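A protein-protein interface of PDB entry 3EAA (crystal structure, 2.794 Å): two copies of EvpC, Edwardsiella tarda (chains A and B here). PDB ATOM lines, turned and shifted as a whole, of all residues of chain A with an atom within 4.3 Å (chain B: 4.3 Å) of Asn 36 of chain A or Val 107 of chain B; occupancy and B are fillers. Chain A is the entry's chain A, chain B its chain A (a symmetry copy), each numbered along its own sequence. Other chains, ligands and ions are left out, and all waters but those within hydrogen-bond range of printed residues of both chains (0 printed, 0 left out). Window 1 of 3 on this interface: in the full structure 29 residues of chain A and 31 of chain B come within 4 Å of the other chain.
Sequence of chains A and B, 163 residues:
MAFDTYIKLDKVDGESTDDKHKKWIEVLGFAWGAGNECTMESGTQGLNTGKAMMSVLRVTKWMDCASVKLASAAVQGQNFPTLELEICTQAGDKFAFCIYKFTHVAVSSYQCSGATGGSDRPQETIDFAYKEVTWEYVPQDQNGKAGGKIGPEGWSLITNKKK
Of the printed residues of chain B, Asn 36 of chain A touches Ala 74 (2.7 Å), Gly 77 (3.9 Å), Val 107 (2.9 Å) and Ser 108 (2.9 Å).
Val 107 of chain B touches just one residue of chain A: Asn 36.
Printed residues of chain A within 4 Å of Gly 77 of chain B: Asn 36 and Thr 49.
Of the printed residues of chain A, Ser 109 of chain B touches Gly 35.
Of the printed residues of chain B, Thr 49 of chain A touches Gly 77.
Printed residues of chain A within 4 Å of Ala 74 of chain B: Gly 35 and Asn 36.
Leu 70 of chain B touches none of the printed residues of chain A.
The nearest printed residue of chain A that does not touch Val 107 of chain B is Gly 35 of chain A (5.3 Å).
The nearest printed residue of chain B that does not touch Gly 35 of chain A is Val 107 of chain B (5.3 Å).
The backbone carbonyl oxygen (O) of Ser 109 of chain B sits at hydrogen-bond distance from the backbone NH (N) of Asp 127 of chain B, 3.1 Å away.
The backbone carbonyl oxygen of Asp 127 of chain B is in hydrogen-bond range of the backbone NH of Ser 108 of chain B (2.8 Å).
OD1 of Asn 36 of chain A lies close to OG1 of Thr 49 of chain A, 2.9 Å away.
The backbone NH (N) of Cys 38 of chain A lies close to the side-chain amide oxygen (OD1) of Asn 36 of chain A, 3.2 Å away.
The backbone NH (N) of Glu 37 of chain A sits at hydrogen-bond distance from the backbone carbonyl oxygen (O) of Thr 49 of chain A.
No position is printed for both chains.
Of the 11 printed residues of chain B, 5 touch a printed residue of chain A.
Among the printed residues, merely in contact across the chains: Gly 35 of chain A with Ala 74 of chain B (3.8 Å), Gly 35 of chain A with Ser 108 of chain B (3.3 Å), Gly 35 of chain A with Ser 109 of chain B (3.6 Å), Asn 36 of chain A with Gly 77 of chain B (3.9 Å), Cys 38 of chain A with Ser 108 of chain B (3.98 Å) and Thr 49 of chain A with Gly 77 of chain B (3.3 Å).
The side-chain amide nitrogen (ND2) of Asn 36 of chain A sits at hydrogen-bond distance from the backbone carbonyl oxygen (O) of Val 107 of chain B (2.9 Å).
ND2 of Asn 36 of chain A lies within hydrogen-bond range of O of Ala 74 of chain B, at 2.7 Å.
N of Asn 36 of chain A is in hydrogen-bond range of O of Ser 108 of chain B, at 2.9 Å.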
ATOM      1  N   GLY A  35      10.586  17.573  10.169  1.00  0.00           N
ATOM      2  CA  GLY A  35      10.186  18.835  10.747  1.00  0.00           C
ATOM      3  C   GLY A  35       9.127  18.575  11.788  1.00  0.00           C
ATOM      4  O   GLY A  35       8.490  17.525  11.771  1.00  0.00           O
ATOM      5  N   ASN A  36       8.945  19.523  12.696  1.00  0.00           N
ATOM      6  CA  ASN A  36       8.005  19.340  13.784  1.00  0.00           C
ATOM      7  C   ASN A  36       6.704  20.110  13.571  1.00  0.00           C
ATOM      8  O   ASN A  36       6.500  20.731  12.529  1.00  0.00           O
ATOM      9  CB  ASN A  36       8.658  19.701  15.116  1.00  0.00           C
ATOM     10  CG  ASN A  36       9.183  21.099  15.139  1.00  0.00           C
ATOM     11  OD1 ASN A  36       8.433  22.053  15.325  1.00  0.00           O
ATOM     12  ND2 ASN A  36      10.485  21.237  14.959  1.00  0.00           N
ATOM     13  N   GLU A  37       5.810  20.045  14.547  1.00  0.00           N
ATOM     14  CA  GLU A  37       4.525  20.721  14.418  1.00  0.00           C
ATOM     15  C   GLU A  37       4.489  22.059  15.159  1.00  0.00           C
ATOM     16  O   GLU A  37       3.661  22.285  16.046  1.00  0.00           O
ATOM     17  CB  GLU A  37       3.373  19.806  14.845  1.00  0.00           C
ATOM     18  CG  GLU A  37       3.600  19.056  16.151  1.00  0.00           C
ATOM     19  CD  GLU A  37       2.329  18.426  16.690  1.00  0.00           C
ATOM     20  OE1 GLU A  37       2.147  18.423  17.921  1.00  0.00           O
ATOM     21  OE2 GLU A  37       1.507  17.948  15.880  1.00  0.00           O
ATOM     22  N   CYS A  38       5.398  22.945  14.765  1.00  0.00           N
ATOM     23  CA  CYS A  38       5.479  24.281  15.335  1.00  0.00           C
ATOM     24  C   CYS A  38       4.543  25.234  14.606  1.00  0.00           C
ATOM     25  O   CYS A  38       4.751  25.555  13.436  1.00  0.00           O
ATOM     26  CB  CYS A  38       6.915  24.806  15.273  1.00  0.00           C
ATOM     27  SG  CYS A  38       7.214  26.180  16.400  1.00  0.00           S
ATOM     28  N   THR A  49       6.849  23.199  20.149  1.00  0.00           N
ATOM     29  CA  THR A  49       7.303  22.395  19.017  1.00  0.00           C
ATOM     30  C   THR A  49       6.455  21.148  18.789  1.00  0.00           C
ATOM     31  O   THR A  49       6.400  20.611  17.674  1.00  0.00           O
ATOM     32  CB  THR A  49       8.750  21.931  19.221  1.00  0.00           C
ATOM     33  OG1 THR A  49       9.190  21.242  18.050  1.00  0.00           O
ATOM     34  CG2 THR A  49       8.842  20.982  20.403  1.00  0.00           C
ATOM     35  N   LYS A  51       5.338  17.551  18.378  1.00  0.00           N
ATOM     36  CA  LYS A  51       5.894  16.299  18.071  1.00  0.00           C
ATOM     37  C   LYS A  51       6.765  16.419  16.924  1.00  0.00           C
ATOM     38  O   LYS A  51       6.600  17.249  16.125  1.00  0.00           O
ATOM     39  CB  LYS A  51       4.766  15.433  17.642  1.00  0.00           C
ATOM     40  CG  LYS A  51       4.682  14.177  18.248  1.00  0.00           C
ATOM     41  CD  LYS A  51       5.021  13.208  17.275  1.00  0.00           C
ATOM     42  CE  LYS A  51       6.089  12.380  17.724  1.00  0.00           C
ATOM     43  NZ  LYS A  51       6.708  11.800  16.575  1.00  0.00           N
ATOM     44  N   LEU B  70      20.741  21.749  10.971  1.00  0.00           N
ATOM     45  CA  LEU B  70      19.401  22.123  10.563  1.00  0.00           C
ATOM     46  C   LEU B  70      18.525  20.902  10.624  1.00  0.00           C
ATOM     47  O   LEU B  70      17.383  20.961  11.079  1.00  0.00           O
ATOM     48  CB  LEU B  70      19.422  22.707   9.153  1.00  0.00           C
ATOM     49  CG  LEU B  70      20.374  23.908   9.141  1.00  0.00           C
ATOM     50  CD1 LEU B  70      20.806  24.332   7.749  1.00  0.00           C
ATOM     51  CD2 LEU B  70      19.764  25.076   9.906  1.00  0.00           C
ATOM     52  N   ALA B  73      17.947  20.156  14.233  1.00  0.00           N
ATOM     53  CA  ALA B  73      17.098  21.170  14.822  1.00  0.00           C
ATOM     54  C   ALA B  73      15.635  20.783  14.620  1.00  0.00           C
ATOM     55  O   ALA B  73      14.843  20.769  15.565  1.00  0.00           O
ATOM     56  CB  ALA B  73      17.396  22.537  14.229  1.00  0.00           C
ATOM     57  N   ALA B  74      15.286  20.444  13.385  1.00  0.00           N
ATOM     58  CA  ALA B  74      13.924  20.034  13.077  1.00  0.00           C
ATOM     59  C   ALA B  74      13.362  19.075  14.136  1.00  0.00           C
ATOM     60  O   ALA B  74      12.518  19.465  14.943  1.00  0.00           O
ATOM     61  CB  ALA B  74      13.858  19.408  11.706  1.00  0.00           C
ATOM     62  N   GLY B  77      13.257  20.099  17.875  1.00  0.00           N
ATOM     63  CA  GLY B  77      12.505  21.265  18.287  1.00  0.00           C
ATOM     64  C   GLY B  77      13.409  22.321  18.885  1.00  0.00           C
ATOM     65  O   GLY B  77      13.036  23.006  19.826  1.00  0.00           O
ATOM     66  N   ALA B 106      12.758  28.725  15.728  1.00  0.00           N
ATOM     67  CA  ALA B 106      12.829  27.268  15.618  1.00  0.00           C
ATOM     68  C   ALA B 106      12.842  26.833  14.152  1.00  0.00           C
ATOM     69  O   ALA B 106      12.380  27.551  13.278  1.00  0.00           O
ATOM     70  CB  ALA B 106      11.651  26.629  16.345  1.00  0.00           C
ATOM     71  N   VAL B 107      13.371  25.651  13.880  1.00  0.00           N
ATOM     72  CA  VAL B 107      13.175  25.039  12.572  1.00  0.00           C
ATOM     73  C   VAL B 107      11.904  24.191  12.612  1.00  0.00           C
ATOM     74  O   VAL B 107      11.836  23.198  13.337  1.00  0.00           O
ATOM     75  CB  VAL B 107      14.367  24.150  12.149  1.00  0.00           C
ATOM     76  CG1 VAL B 107      14.060  23.483  10.823  1.00  0.00           C
ATOM     77  CG2 VAL B 107      15.651  24.958  12.062  1.00  0.00           C
ATOM     78  N   SER B 108      10.894  24.586  11.844  1.00  0.00           N
ATOM     79  CA  SER B 108       9.611  23.891  11.869  1.00  0.00           C
ATOM     80  C   SER B 108       9.588  22.761  10.849  1.00  0.00           C
ATOM     81  O   SER B 108       8.820  21.812  10.963  1.00  0.00           O
ATOM     82  CB  SER B 108       8.461  24.866  11.607  1.00  0.00           C
ATOM     83  OG  SER B 108       8.729  25.695  10.485  1.00  0.00           O
ATOM     84  N   SER B 109      10.435  22.874   9.841  1.00  0.00           N
ATOM     85  CA  SER B 109      10.562  21.819   8.860  1.00  0.00           C
ATOM     86  C   SER B 109      11.885  21.940   8.139  1.00  0.00           C
ATOM     87  O   SER B 109      12.432  23.029   7.949  1.00  0.00           O
ATOM     88  CB  SER B 109       9.424  21.862   7.847  1.00  0.00           C
ATOM     89  OG  SER B 109       9.761  22.680   6.739  1.00  0.00           O
ATOM     90  N   ILE B 126      14.101  25.211   4.074  1.00  0.00           N
ATOM     91  CA  ILE B 126      13.888  25.269   5.513  1.00  0.00           C
ATOM     92  C   ILE B 126      12.835  26.289   5.950  1.00  0.00           C
ATOM     93  O   ILE B 126      12.838  27.447   5.518  1.00  0.00           O
ATOM     94  CB  ILE B 126      15.186  25.587   6.275  1.00  0.00           C
ATOM     95  CG1 ILE B 126      16.310  24.652   5.854  1.00  0.00           C
ATOM     96  CG2 ILE B 126      14.952  25.479   7.766  1.00  0.00           C
ATOM     97  CD1 ILE B 126      17.108  25.170   4.708  1.00  0.00           C
ATOM     98  N   ASP B 127      11.943  25.853   6.832  1.00  0.00           N
ATOM     99  CA  ASP B 127      10.946  26.741   7.395  1.00  0.00           C
ATOM    100  C   ASP B 127      11.303  27.101   8.829  1.00  0.00           C
ATOM    101  O   ASP B 127      11.471  26.234   9.686  1.00  0.00           O
ATOM    102  CB  ASP B 127       9.548  26.124   7.303  1.00  0.00           C
ATOM    103  CG  ASP B 127       8.952  26.234   5.902  1.00  0.00           C
ATOM    104  OD1 ASP B 127       9.703  26.559   4.958  1.00  0.00           O
ATOM    105  OD2 ASP B 127       7.729  26.017   5.742  1.00  0.00           O
ATOM    106  N   PHE B 128      11.423  28.401   9.066  1.00  0.00           N
ATOM    107  CA  PHE B 128      11.812  28.931  10.355  1.00  0.00           C
ATOM    108  C   PHE B 128      10.637  29.579  11.067  1.00  0.00           C
ATOM    109  O   PHE B 128      10.171  30.648  10.668  1.00  0.00           O
ATOM    110  CB  PHE B 128      12.904  29.965  10.166  1.00  0.00           C
ATOM    111  CG  PHE B 128      14.240  29.383   9.844  1.00  0.00           C
ATOM    112  CD1 PHE B 128      14.763  29.498   8.580  1.00  0.00           C
ATOM    113  CD2 PHE B 128      14.982  28.740  10.814  1.00  0.00           C
ATOM    114  CE1 PHE B 128      16.001  28.978   8.283  1.00  0.00           C
ATOM    115  CE2 PHE B 128      16.218  28.225  10.526  1.00  0.00           C
ATOM    116  CZ  PHE B 128      16.732  28.341   9.257  1.00  0.00           C
